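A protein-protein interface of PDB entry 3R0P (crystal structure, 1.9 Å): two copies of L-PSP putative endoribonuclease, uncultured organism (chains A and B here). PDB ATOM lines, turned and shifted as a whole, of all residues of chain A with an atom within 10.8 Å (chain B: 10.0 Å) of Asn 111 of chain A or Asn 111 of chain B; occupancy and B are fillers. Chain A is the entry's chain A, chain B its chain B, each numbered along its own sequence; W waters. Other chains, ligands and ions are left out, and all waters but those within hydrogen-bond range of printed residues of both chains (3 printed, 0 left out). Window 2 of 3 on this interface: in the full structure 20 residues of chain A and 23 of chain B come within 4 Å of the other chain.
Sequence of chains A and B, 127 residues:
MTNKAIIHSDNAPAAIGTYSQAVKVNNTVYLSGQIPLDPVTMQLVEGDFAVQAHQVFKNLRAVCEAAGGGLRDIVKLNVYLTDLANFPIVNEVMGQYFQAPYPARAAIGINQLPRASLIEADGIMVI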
ATOM      1  N   VAL A  79      37.124  -4.761  19.994  1.00  0.00           N
ATOM      2  CA  VAL A  79      36.020  -3.878  19.660  1.00  0.00           C
ATOM      3  C   VAL A  79      34.712  -4.649  19.605  1.00  0.00           C
ATOM      4  O   VAL A  79      34.576  -5.593  18.825  1.00  0.00           O
ATOM      5  CB  VAL A  79      36.239  -3.187  18.306  1.00  0.00           C
ATOM      6  CG1 VAL A  79      35.076  -2.247  18.006  1.00  0.00           C
ATOM      7  CG2 VAL A  79      37.576  -2.451  18.299  1.00  0.00           C
ATOM      8  N   TYR A  80      33.763  -4.245  20.446  1.00  0.00           N
ATOM      9  CA  TYR A  80      32.443  -4.868  20.513  1.00  0.00           C
ATOM     10  C   TYR A  80      31.405  -3.925  19.907  1.00  0.00           C
ATOM     11  O   TYR A  80      31.304  -2.761  20.312  1.00  0.00           O
ATOM     12  CB  TYR A  80      32.092  -5.188  21.976  1.00  0.00           C
ATOM     13  CG  TYR A  80      33.139  -6.046  22.649  1.00  0.00           C
ATOM     14  CD1 TYR A  80      33.151  -7.420  22.472  1.00  0.00           C
ATOM     15  CD2 TYR A  80      34.134  -5.479  23.432  1.00  0.00           C
ATOM     16  CE1 TYR A  80      34.119  -8.203  23.069  1.00  0.00           C
ATOM     17  CE2 TYR A  80      35.106  -6.259  24.031  1.00  0.00           C
ATOM     18  CZ  TYR A  80      35.095  -7.615  23.845  1.00  0.00           C
ATOM     19  OH  TYR A  80      36.065  -8.392  24.440  1.00  0.00           O
ATOM     20  N   LEU A  81      30.644  -4.422  18.934  1.00  0.00           N
ATOM     21  CA  LEU A  81      29.616  -3.620  18.273  1.00  0.00           C
ATOM     22  C   LEU A  81      28.273  -4.324  18.375  1.00  0.00           C
ATOM     23  O   LEU A  81      28.195  -5.542  18.246  1.00  0.00           O
ATOM     24  CB  LEU A  81      29.945  -3.426  16.783  1.00  0.00           C
ATOM     25  CG  LEU A  81      31.268  -2.767  16.372  1.00  0.00           C
ATOM     26  CD1 LEU A  81      31.241  -2.391  14.899  1.00  0.00           C
ATOM     27  CD2 LEU A  81      31.544  -1.526  17.207  1.00  0.00           C
ATOM     28  N   THR A  82      27.209  -3.561  18.589  1.00  0.00           N
ATOM     29  CA  THR A  82      25.870  -4.123  18.524  1.00  0.00           C
ATOM     30  C   THR A  82      25.514  -4.474  17.090  1.00  0.00           C
ATOM     31  O   THR A  82      24.678  -5.340  16.855  1.00  0.00           O
ATOM     32  CB  THR A  82      24.824  -3.142  19.069  1.00  0.00           C
ATOM     33  OG1 THR A  82      24.947  -1.894  18.377  1.00  0.00           O
ATOM     34  CG2 THR A  82      25.054  -2.914  20.550  1.00  0.00           C
ATOM     35  N   ASP A  83      26.161  -3.816  16.129  1.00  0.00           N
ATOM     36  CA  ASP A  83      25.882  -4.058  14.712  1.00  0.00           C
ATOM     37  C   ASP A  83      27.150  -3.928  13.865  1.00  0.00           C
ATOM     38  O   ASP A  83      27.699  -2.835  13.734  1.00  0.00           O
ATOM     39  CB  ASP A  83      24.813  -3.076  14.209  1.00  0.00           C
ATOM     40  CG  ASP A  83      24.275  -3.445  12.818  1.00  0.00           C
ATOM     41  OD1 ASP A  83      24.919  -4.243  12.103  1.00  0.00           O
ATOM     42  OD2 ASP A  83      23.203  -2.928  12.439  1.00  0.00           O
ATOM     43  N   LEU A  84      27.609  -5.032  13.278  1.00  0.00           N
ATOM     44  CA  LEU A  84      28.840  -4.998  12.486  1.00  0.00           C
ATOM     45  C   LEU A  84      28.702  -4.206  11.192  1.00  0.00           C
ATOM     46  O   LEU A  84      29.698  -3.916  10.528  1.00  0.00           O
ATOM     47  CB  LEU A  84      29.359  -6.409  12.181  1.00  0.00           C
ATOM     48  CG  LEU A  84      29.990  -7.150  13.356  1.00  0.00           C
ATOM     49  CD1 LEU A  84      30.608  -8.456  12.874  1.00  0.00           C
ATOM     50  CD2 LEU A  84      31.029  -6.276  14.062  1.00  0.00           C
ATOM     51  N   ILE A 108      34.041  -7.991  17.251  1.00  0.00           N
ATOM     52  CA  ILE A 108      32.975  -8.928  17.560  1.00  0.00           C
ATOM     53  C   ILE A 108      31.612  -8.253  17.575  1.00  0.00           C
ATOM     54  O   ILE A 108      31.441  -7.194  18.184  1.00  0.00           O
ATOM     55  CB  ILE A 108      33.187  -9.555  18.960  1.00  0.00           C
ATOM     56  CG1 ILE A 108      34.633 -10.013  19.130  1.00  0.00           C
ATOM     57  CG2 ILE A 108      32.221 -10.702  19.185  1.00  0.00           C
ATOM     58  CD1 ILE A 108      35.073 -11.012  18.072  1.00  0.00           C
ATOM     59  N   GLY A 109      30.635  -8.889  16.942  1.00  0.00           N
ATOM     60  CA  GLY A 109      29.267  -8.410  16.980  1.00  0.00           C
ATOM     61  C   GLY A 109      28.559  -9.042  18.162  1.00  0.00           C
ATOM     62  O   GLY A 109      28.384 -10.260  18.216  1.00  0.00           O
ATOM     63  N   ILE A 110      28.154  -8.219  19.122  1.00  0.00           N
ATOM     64  CA  ILE A 110      27.515  -8.740  20.328  1.00  0.00           C
ATOM     65  C   ILE A 110      26.065  -8.284  20.452  1.00  0.00           C
ATOM     66  O   ILE A 110      25.530  -7.636  19.553  1.00  0.00           O
ATOM     67  CB  ILE A 110      28.328  -8.422  21.601  1.00  0.00           C
ATOM     68  CG1 ILE A 110      28.773  -6.960  21.624  1.00  0.00           C
ATOM     69  CG2 ILE A 110      29.562  -9.302  21.665  1.00  0.00           C
ATOM     70  CD1 ILE A 110      27.646  -5.968  21.744  1.00  0.00           C
ATOM     71  N   ASN A 111      25.425  -8.639  21.559  1.00  0.00           N
ATOM     72  CA  ASN A 111      23.998  -8.384  21.704  1.00  0.00           C
ATOM     73  C   ASN A 111      23.668  -7.047  22.347  1.00  0.00           C
ATOM     74  O   ASN A 111      22.832  -6.298  21.839  1.00  0.00           O
ATOM     75  CB  ASN A 111      23.318  -9.507  22.476  1.00  0.00           C
ATOM     76  CG  ASN A 111      21.824  -9.336  22.535  1.00  0.00           C
ATOM     77  OD1 ASN A 111      21.140  -9.403  21.513  1.00  0.00           O
ATOM     78  ND2 ASN A 111      21.301  -9.117  23.732  1.00  0.00           N
ATOM     79  N   GLN A 112      24.313  -6.750  23.468  1.00  0.00           N
ATOM     80  CA  GLN A 112      24.081  -5.471  24.129  1.00  0.00           C
ATOM     81  C   GLN A 112      25.296  -4.976  24.908  1.00  0.00           C
ATOM     82  O   GLN A 112      26.185  -5.751  25.259  1.00  0.00           O
ATOM     83  CB  GLN A 112      22.835  -5.521  25.019  1.00  0.00           C
ATOM     84  CG  GLN A 112      22.713  -6.771  25.848  1.00  0.00           C
ATOM     85  CD  GLN A 112      21.604  -6.677  26.885  1.00  0.00           C
ATOM     86  OE1 GLN A 112      20.905  -5.662  26.978  1.00  0.00           O
ATOM     87  NE2 GLN A 112      21.445  -7.734  27.675  1.00  0.00           N
ATOM     88  N   LEU A 113      25.324  -3.673  25.167  1.00  0.00           N
ATOM     89  CA  LEU A 113      26.443  -3.061  25.853  1.00  0.00           C
ATOM     90  C   LEU A 113      25.919  -2.172  26.958  1.00  0.00           C
ATOM     91  O   LEU A 113      24.748  -1.800  26.942  1.00  0.00           O
ATOM     92  CB  LEU A 113      27.274  -2.240  24.867  1.00  0.00           C
ATOM     93  CG  LEU A 113      28.026  -3.045  23.802  1.00  0.00           C
ATOM     94  CD1 LEU A 113      28.659  -2.111  22.781  1.00  0.00           C
ATOM     95  CD2 LEU A 113      29.080  -3.949  24.443  1.00  0.00           C
ATOM     96  N   PRO A 114      26.779  -1.830  27.927  1.00  0.00           N
ATOM     97  CA  PRO A 114      26.349  -0.905  28.984  1.00  0.00           C
ATOM     98  C   PRO A 114      25.770   0.393  28.413  1.00  0.00           C
ATOM     99  O   PRO A 114      26.249   0.910  27.390  1.00  0.00           O
ATOM    100  CB  PRO A 114      27.645  -0.628  29.760  1.00  0.00           C
ATOM    101  CG  PRO A 114      28.469  -1.860  29.549  1.00  0.00           C
ATOM    102  CD  PRO A 114      28.157  -2.313  28.136  1.00  0.00           C
ATOM    103  N   ARG A 115      24.733   0.900  29.074  1.00  0.00           N
ATOM    104  CA  ARG A 115      24.091   2.161  28.698  1.00  0.00           C
ATOM    105  C   ARG A 115      23.543   2.145  27.274  1.00  0.00           C
ATOM    106  O   ARG A 115      23.307   3.200  26.694  1.00  0.00           O
ATOM    107  CB  ARG A 115      25.056   3.343  28.859  1.00  0.00           C
ATOM    108  CG  ARG A 115      25.821   3.358  30.162  1.00  0.00           C
ATOM    109  CD  ARG A 115      24.906   3.540  31.359  1.00  0.00           C
ATOM    110  NE  ARG A 115      25.324   4.695  32.141  1.00  0.00           N
ATOM    111  CZ  ARG A 115      24.804   5.907  32.010  1.00  0.00           C
ATOM    112  NH1 ARG A 115      23.826   6.127  31.140  1.00  0.00           N
ATOM    113  NH2 ARG A 115      25.254   6.898  32.757  1.00  0.00           N
ATOM    114  N   ALA A 116      23.342   0.953  26.717  1.00  0.00           N
ATOM    115  CA  ALA A 116      22.781   0.817  25.376  1.00  0.00           C
ATOM    116  C   ALA A 116      23.715   1.386  24.306  1.00  0.00           C
ATOM    117  O   ALA A 116      23.280   1.767  23.217  1.00  0.00           O
ATOM    118  CB  ALA A 116      21.408   1.477  25.304  1.00  0.00           C
ATOM    119  N   SER A 117      25.001   1.434  24.630  1.00  0.00           N
ATOM    120  CA  SER A 117      26.030   1.879  23.700  1.00  0.00           C
ATOM    121  C   SER A 117      26.061   1.044  22.408  1.00  0.00           C
ATOM    122  O   SER A 117      25.644  -0.120  22.389  1.00  0.00           O
ATOM    123  CB  SER A 117      27.397   1.837  24.392  1.00  0.00           C
ATOM    124  OG  SER A 117      27.379   2.588  25.602  1.00  0.00           O
ATOM    125  N   LEU A 118      26.566   1.642  21.335  1.00  0.00           N
ATOM    126  CA  LEU A 118      26.687   0.940  20.063  1.00  0.00           C
ATOM    127  C   LEU A 118      28.077   0.343  19.898  1.00  0.00           C
ATOM    128  O   LEU A 118      28.312  -0.475  19.001  1.00  0.00           O
ATOM    129  CB  LEU A 118      26.397   1.884  18.891  1.00  0.00           C
ATOM    130  CG  LEU A 118      25.051   2.612  18.928  1.00  0.00           C
ATOM    131  CD1 LEU A 118      24.970   3.610  17.780  1.00  0.00           C
ATOM    132  CD2 LEU A 118      23.902   1.620  18.862  1.00  0.00           C
ATOM    133  N   ILE A 119      28.998   0.769  20.753  1.00  0.00           N
ATOM    134  CA  ILE A 119      30.385   0.331  20.668  1.00  0.00           C
ATOM    135  C   ILE A 119      31.065   0.414  22.032  1.00  0.00           C
ATOM    136  O   ILE A 119      30.850   1.359  22.799  1.00  0.00           O
ATOM    137  CB  ILE A 119      31.187   1.167  19.650  1.00  0.00           C
ATOM    138  CG1 ILE A 119      32.686   0.863  19.748  1.00  0.00           C
ATOM    139  CG2 ILE A 119      30.946   2.683  19.849  1.00  0.00           C
ATOM    140  CD1 ILE A 119      33.522   1.518  18.625  1.00  0.00           C
ATOM    141  N   GLU A 120      31.868  -0.599  22.337  1.00  0.00           N
ATOM    142  CA  GLU A 120      32.727  -0.583  23.503  1.00  0.00           C
ATOM    143  C   GLU A 120      34.068  -1.123  23.049  1.00  0.00           C
ATOM    144  O   GLU A 120      34.117  -2.033  22.231  1.00  0.00           O
ATOM    145  CB  GLU A 120      32.142  -1.476  24.598  1.00  0.00           C
ATOM    146  CG  GLU A 120      33.032  -1.611  25.833  1.00  0.00           C
ATOM    147  CD  GLU A 120      32.360  -2.406  26.942  1.00  0.00           C
ATOM    148  OE1 GLU A 120      31.124  -2.546  26.895  1.00  0.00           O
ATOM    149  OE2 GLU A 120      33.063  -2.897  27.851  1.00  0.00           O
ATOM    150  N   TYR B  80      31.034 -11.914  30.841  1.00  0.00           N
ATOM    151  CA  TYR B  80      30.092 -12.144  29.747  1.00  0.00           C
ATOM    152  C   TYR B  80      28.722 -12.519  30.307  1.00  0.00           C
ATOM    153  O   TYR B  80      28.592 -13.509  31.022  1.00  0.00           O
ATOM    154  CB  TYR B  80      30.609 -13.259  28.825  1.00  0.00           C
ATOM    155  CG  TYR B  80      31.965 -12.949  28.231  1.00  0.00           C
ATOM    156  CD1 TYR B  80      32.090 -12.066  27.167  1.00  0.00           C
ATOM    157  CD2 TYR B  80      33.120 -13.517  28.753  1.00  0.00           C
ATOM    158  CE1 TYR B  80      33.338 -11.771  26.618  1.00  0.00           C
ATOM    159  CE2 TYR B  80      34.371 -13.228  28.211  1.00  0.00           C
ATOM    160  CZ  TYR B  80      34.472 -12.355  27.155  1.00  0.00           C
ATOM    161  OH  TYR B  80      35.712 -12.068  26.634  1.00  0.00           O
ATOM    162  N   LEU B  81      27.701 -11.737  29.979  1.00  0.00           N
ATOM    163  CA  LEU B  81      26.370 -11.977  30.534  1.00  0.00           C
ATOM    164  C   LEU B  81      25.357 -12.158  29.406  1.00  0.00           C
ATOM    165  O   LEU B  81      25.464 -11.510  28.366  1.00  0.00           O
ATOM    166  CB  LEU B  81      25.928 -10.813  31.433  1.00  0.00           C
ATOM    167  CG  LEU B  81      26.751 -10.374  32.648  1.00  0.00           C
ATOM    168  CD1 LEU B  81      26.037  -9.251  33.397  1.00  0.00           C
ATOM    169  CD2 LEU B  81      27.026 -11.537  33.587  1.00  0.00           C
ATOM    170  N   THR B  82      24.374 -13.034  29.606  1.00  0.00           N
ATOM    171  CA  THR B  82      23.299 -13.177  28.624  1.00  0.00           C
ATOM    172  C   THR B  82      22.273 -12.050  28.740  1.00  0.00           C
ATOM    173  O   THR B  82      21.496 -11.823  27.816  1.00  0.00           O
ATOM    174  CB  THR B  82      22.569 -14.529  28.749  1.00  0.00           C
ATOM    175  OG1 THR B  82      22.047 -14.660  30.075  1.00  0.00           O
ATOM    176  CG2 THR B  82      23.517 -15.686  28.448  1.00  0.00           C
ATOM    177  N   ASP B  83      22.269 -11.359  29.881  1.00  0.00           N
ATOM    178  CA  ASP B  83      21.419 -10.192  30.080  1.00  0.00           C
ATOM    179  C   ASP B  83      22.159  -9.176  30.942  1.00  0.00           C
ATOM    180  O   ASP B  83      22.418  -9.426  32.122  1.00  0.00           O
ATOM    181  CB  ASP B  83      20.103 -10.590  30.758  1.00  0.00           C
ATOM    182  CG  ASP B  83      19.068  -9.469  30.740  1.00  0.00           C
ATOM    183  OD1 ASP B  83      19.442  -8.302  30.491  1.00  0.00           O
ATOM    184  OD2 ASP B  83      17.875  -9.754  30.983  1.00  0.00           O
ATOM    185  N   LEU B  84      22.503  -8.029  30.360  1.00  0.00           N
ATOM    186  CA  LEU B  84      23.248  -7.006  31.096  1.00  0.00           C
ATOM    187  C   LEU B  84      22.464  -6.407  32.250  1.00  0.00           C
ATOM    188  O   LEU B  84      23.023  -5.679  33.073  1.00  0.00           O
ATOM    189  CB  LEU B  84      23.716  -5.887  30.170  1.00  0.00           C
ATOM    190  CG  LEU B  84      25.017  -6.139  29.423  1.00  0.00           C
ATOM    191  CD1 LEU B  84      25.447  -4.855  28.737  1.00  0.00           C
ATOM    192  CD2 LEU B  84      26.101  -6.622  30.368  1.00  0.00           C
ATOM    193  N   ALA B  85      21.168  -6.691  32.297  1.00  0.00           N
ATOM    194  CA  ALA B  85      20.335  -6.219  33.391  1.00  0.00           C
ATOM    195  C   ALA B  85      20.858  -6.814  34.687  1.00  0.00           C
ATOM    196  O   ALA B  85      20.642  -6.270  35.766  1.00  0.00           O
ATOM    197  CB  ALA B  85      18.884  -6.618  33.164  1.00  0.00           C
ATOM    198  N   ALA B 107      32.515  -5.567  30.491  1.00  0.00           N
ATOM    199  CA  ALA B 107      31.259  -6.285  30.658  1.00  0.00           C
ATOM    200  C   ALA B 107      30.480  -6.236  29.358  1.00  0.00           C
ATOM    201  O   ALA B 107      30.194  -5.160  28.832  1.00  0.00           O
ATOM    202  CB  ALA B 107      30.445  -5.685  31.780  1.00  0.00           C
ATOM    203  N   ILE B 108      30.144  -7.409  28.833  1.00  0.00           N
ATOM    204  CA  ILE B 108      29.542  -7.488  27.514  1.00  0.00           C
ATOM    205  C   ILE B 108      28.280  -8.334  27.550  1.00  0.00           C
ATOM    206  O   ILE B 108      28.260  -9.398  28.173  1.00  0.00           O
ATOM    207  CB  ILE B 108      30.510  -8.173  26.525  1.00  0.00           C
ATOM    208  CG1 ILE B 108      31.926  -7.617  26.688  1.00  0.00           C
ATOM    209  CG2 ILE B 108      30.011  -8.016  25.102  1.00  0.00           C
ATOM    210  CD1 ILE B 108      32.027  -6.136  26.365  1.00  0.00           C
ATOM    211  N   GLY B 109      27.238  -7.876  26.862  1.00  0.00           N
ATOM    212  CA  GLY B 109      26.016  -8.650  26.732  1.00  0.00           C
ATOM    213  C   GLY B 109      26.083  -9.531  25.499  1.00  0.00           C
ATOM    214  O   GLY B 109      26.119  -9.036  24.374  1.00  0.00           O
ATOM    215  N   ILE B 110      26.092 -10.844  25.715  1.00  0.00           N
ATOM    216  CA  ILE B 110      26.295 -11.791  24.628  1.00  0.00           C
ATOM    217  C   ILE B 110      25.067 -12.687  24.442  1.00  0.00           C
ATOM    218  O   ILE B 110      24.052 -12.494  25.116  1.00  0.00           O
ATOM    219  CB  ILE B 110      27.609 -12.592  24.825  1.00  0.00           C
ATOM    220  CG1 ILE B 110      27.712 -13.173  26.240  1.00  0.00           C
ATOM    221  CG2 ILE B 110      28.799 -11.666  24.624  1.00  0.00           C
ATOM    222  CD1 ILE B 110      26.606 -14.136  26.617  1.00  0.00           C
ATOM    223  N   ASN B 111      25.157 -13.652  23.526  1.00  0.00           N
ATOM    224  CA  ASN B 111      23.995 -14.435  23.109  1.00  0.00           C
ATOM    225  C   ASN B 111      23.833 -15.780  23.828  1.00  0.00           C
ATOM    226  O   ASN B 111      22.736 -16.134  24.259  1.00  0.00           O
ATOM    227  CB  ASN B 111      24.023 -14.647  21.585  1.00  0.00           C
ATOM    228  CG  ASN B 111      23.828 -13.342  20.802  1.00  0.00           C
ATOM    229  OD1 ASN B 111      22.820 -13.164  20.115  1.00  0.00           O
ATOM    230  ND2 ASN B 111      24.791 -12.424  20.911  1.00  0.00           N
ATOM    231  N   GLN B 112      24.918 -16.536  23.938  1.00  0.00           N
ATOM    232  CA  GLN B 112      24.874 -17.841  24.589  1.00  0.00           C
ATOM    233  C   GLN B 112      26.156 -18.098  25.347  1.00  0.00           C
ATOM    234  O   GLN B 112      27.225 -17.625  24.960  1.00  0.00           O
ATOM    235  CB  GLN B 112      24.738 -18.977  23.569  1.00  0.00           C
ATOM    236  CG  GLN B 112      23.541 -18.938  22.647  1.00  0.00           C
ATOM    237  CD  GLN B 112      23.613 -20.049  21.598  1.00  0.00           C
ATOM    238  OE1 GLN B 112      22.835 -21.002  21.632  1.00  0.00           O
ATOM    239  NE2 GLN B 112      24.558 -19.932  20.672  1.00  0.00           N
ATOM    240  N   LEU B 113      26.045 -18.890  26.407  1.00  0.00           N
ATOM    241  CA  LEU B 113      27.205 -19.360  27.144  1.00  0.00           C
ATOM    242  C   LEU B 113      27.104 -20.872  27.316  1.00  0.00           C
ATOM    243  O   LEU B 113      26.008 -21.430  27.266  1.00  0.00           O
ATOM    244  CB  LEU B 113      27.256 -18.685  28.511  1.00  0.00           C
ATOM    245  CG  LEU B 113      27.458 -17.173  28.495  1.00  0.00           C
ATOM    246  CD1 LEU B 113      27.338 -16.616  29.918  1.00  0.00           C
ATOM    247  CD2 LEU B 113      28.803 -16.831  27.866  1.00  0.00           C
ATOM    248  N   PRO B 114      28.248 -21.542  27.505  1.00  0.00           N
ATOM    249  CA  PRO B 114      28.230 -22.992  27.729  1.00  0.00           C
ATOM    250  C   PRO B 114      27.264 -23.377  28.845  1.00  0.00           C
ATOM    251  O   PRO B 114      27.172 -22.660  29.844  1.00  0.00           O
ATOM    252  CB  PRO B 114      29.672 -23.290  28.138  1.00  0.00           C
ATOM    253  CG  PRO B 114      30.472 -22.267  27.389  1.00  0.00           C
ATOM    254  CD  PRO B 114      29.619 -21.018  27.364  1.00  0.00           C
ATOM    255  N   ARG B 115      26.546 -24.486  28.666  1.00  0.00           N
ATOM    256  CA  ARG B 115      25.602 -24.987  29.667  1.00  0.00           C
ATOM    257  C   ARG B 115      24.435 -24.036  29.936  1.00  0.00           C
ATOM    258  O   ARG B 115      23.777 -24.141  30.972  1.00  0.00           O
ATOM    259  CB  ARG B 115      26.311 -25.279  30.991  1.00  0.00           C
ATOM    260  CG  ARG B 115      27.534 -26.168  30.882  1.00  0.00           C
ATOM    261  CD  ARG B 115      27.164 -27.612  30.612  1.00  0.00           C
ATOM    262  NE  ARG B 115      28.284 -28.506  30.892  1.00  0.00           N
ATOM    263  CZ  ARG B 115      28.336 -29.341  31.924  1.00  0.00           C
ATOM    264  NH1 ARG B 115      27.319 -29.414  32.776  1.00  0.00           N
ATOM    265  NH2 ARG B 115      29.400 -30.112  32.100  1.00  0.00           N
ATOM    266  N   ALA B 116      24.175 -23.115  29.013  1.00  0.00           N
ATOM    267  CA  ALA B 116      23.093 -22.147  29.207  1.00  0.00           C
ATOM    268  C   ALA B 116      23.320 -21.278  30.444  1.00  0.00           C
ATOM    269  O   ALA B 116      22.364 -20.807  31.074  1.00  0.00           O
ATOM    270  CB  ALA B 116      21.752 -22.861  29.301  1.00  0.00           C
ATOM    271  N   SER B 117      24.587 -21.062  30.789  1.00  0.00           N
ATOM    272  CA  SER B 117      24.933 -20.213  31.932  1.00  0.00           C
ATOM    273  C   SER B 117      24.464 -18.774  31.729  1.00  0.00           C
ATOM    274  O   SER B 117      24.301 -18.317  30.596  1.00  0.00           O
ATOM    275  CB  SER B 117      26.444 -20.228  32.175  1.00  0.00           C
ATOM    276  OG  SER B 117      26.921 -21.543  32.391  1.00  0.00           O
ATOM    277  N   LEU B 118      24.262 -18.058  32.831  1.00  0.00           N
ATOM    278  CA  LEU B 118      23.879 -16.655  32.758  1.00  0.00           C
ATOM    279  C   LEU B 118      25.114 -15.769  32.812  1.00  0.00           C
ATOM    280  O   LEU B 118      25.034 -14.567  32.556  1.00  0.00           O
ATOM    281  CB  LEU B 118      22.932 -16.288  33.906  1.00  0.00           C
ATOM    282  CG  LEU B 118      21.648 -17.114  34.018  1.00  0.00           C
ATOM    283  CD1 LEU B 118      20.764 -16.591  35.152  1.00  0.00           C
ATOM    284  CD2 LEU B 118      20.892 -17.113  32.703  1.00  0.00           C
ATOM    285  N   ILE B 119      26.253 -16.371  33.148  1.00  0.00           N
ATOM    286  CA  ILE B 119      27.481 -15.615  33.358  1.00  0.00           C
ATOM    287  C   ILE B 119      28.710 -16.479  33.163  1.00  0.00           C
ATOM    288  O   ILE B 119      28.757 -17.621  33.609  1.00  0.00           O
ATOM    289  CB  ILE B 119      27.531 -14.955  34.763  1.00  0.00           C
ATOM    290  CG1 ILE B 119      28.911 -14.347  35.021  1.00  0.00           C
ATOM    291  CG2 ILE B 119      27.181 -15.965  35.858  1.00  0.00           C
ATOM    292  CD1 ILE B 119      28.969 -13.458  36.233  1.00  0.00           C
ATOM    293  N   GLU B 120      29.690 -15.929  32.456  1.00  0.00           N
ATOM    294  CA  GLU B 120      31.010 -16.530  32.334  1.00  0.00           C
ATOM    295  C   GLU B 120      32.019 -15.416  32.550  1.00  0.00           C
ATOM    296  O   GLU B 120      31.806 -14.298  32.097  1.00  0.00           O
ATOM    297  CB  GLU B 120      31.210 -17.162  30.953  1.00  0.00           C
ATOM    298  CG  GLU B 120      32.636 -17.678  30.727  1.00  0.00           C
ATOM    299  CD  GLU B 120      32.798 -18.479  29.439  1.00  0.00           C
ATOM    300  OE1 GLU B 120      31.779 -18.885  28.844  1.00  0.00           O
ATOM    301  OE2 GLU B 120      33.954 -18.694  29.015  1.00  0.00           O
HETATM  302  O   HOH W   1      22.887  -9.804  26.054  1.00  0.00           O
HETATM  303  O   HOH W   2      32.148  -2.883  30.275  1.00  0.00           O
HETATM  304  O   HOH W   3      35.857 -10.968  24.393  1.00  0.00           O
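O of Gly 109 of chain B lies within hydrogen-bond range of N of Asn 111 of chain A, at 2.9 Å.
The side-chain amide nitrogen (NE2) of Gln 112 of chain A lies close to the backbone NH (N) of Leu 84 of chain B.
The backbone carbonyl oxygen (O) of Gln 112 of chain A sits at hydrogen-bond distance from the backbone NH (N) of Gly 109 of chain B.
OE1 of Glu 120 of chain A sits close to O of Ala 107 of chain B, at 3.4 Å.
Printed residues of chain B that touch a printed residue of chain A: Asp 83, Leu 84, Ala 107, Ile 108, Gly 109, Ile 110 and Asn 111.
Hydrophobic or aromatic side chains of chain B within 4 Å of the printed part of chain A: Leu 84, Ile 108 and Ile 110.
Along chain B the printed residues that touch a printed residue of chain A span positions 83 to 111.
Hydrophobic or aromatic side chains of chain A that line the printed part of chain B: Tyr 80, Ile 110 and Pro 114.
Among the printed residues, pairs that only touch across the chains: Tyr 80 of chain A with Ile 108 of chain B, Ile 110 of chain A with Ile 108 of chain B, Ile 110 of chain A with Gly 109 of chain B, Ile 110 of chain A with Ile 110 of chain B, Asn 111 of chain A with Asn 111 of chain B, Gln 112 of chain A with Asp 83 of chain B, Leu 113 of chain A with Leu 84 of chain B, Pro 114 of chain A with Leu 84 of chain B, Pro 114 of chain A with Ala 107 of chain B and Glu 120 of chain A with Ile 108 of chain B.
O of Glu 120 of chain A is in hydrogen-bond range of N of Tyr 80 of chain A (2.9 Å).
O of Leu 81 of chain A is in hydrogen-bond range of N of Ile 110 of chain A, at 2.8 Å.
O of Pro 114 of chain A is in hydrogen-bond range of OG of Ser 117 of chain A, 2.7 Å away.
N of Leu 81 of chain B sits at hydrogen-bond distance from O of Ile 108 of chain B (3.0 Å).
Water W2 bridges OE2 of Glu 120 of chain A (2.6 Å) and N of Ala 107 of chain B (2.7 Å).
Water W1 lies within hydrogen-bond range of the side-chain amide nitrogen (ND2) of Asn 111 of chain A, the side-chain amide nitrogen (NE2) of Gln 112 of chain A, the backbone carbonyl oxygen (O) of Thr 82 of chain B and the backbone carbonyl oxygen (O) of Ile 110 of chain B.
Of chain B, only Ile 108, Gly 109 and Ile 110 come within 4 Å of Ile 110 of chain A.
Asn 111 of chain A touches two residues of chain B.
Of the printed residues of chain A, Asp 83 of chain B touches Gln 112.
Of the printed residues of chain A, Ala 107 of chain B touches Pro 114 and Glu 120.
Printed residues of chain A within 4 Å of Ile 108 of chain B: Tyr 80, Ile 110 and Glu 120.
Asn 111 of chain B touches just one residue of chain A: Asn 111 (3.6 Å).
The nearest residue of chain A that does not touch Asn 111 of chain B is Ile 110 of chain A (4.4 Å).
Ile 110 of chain A touches Gly 109 of chain B, but with the chains exchanged Gly 109 of chain A does not touch Ile 110 of chain B (6.6 Å).
Glu 120 of chain A touches Ile 108 of chain B, but with the chains exchanged Ile 108 of chain A does not touch Glu 120 of chain B (12.7 Å).
Positions printed for both chains: 80, 81, 82, 83, 84, 108, 109, 110, 111, 112, 113, 114, 115, 116, 117, 118, 119 and 120.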
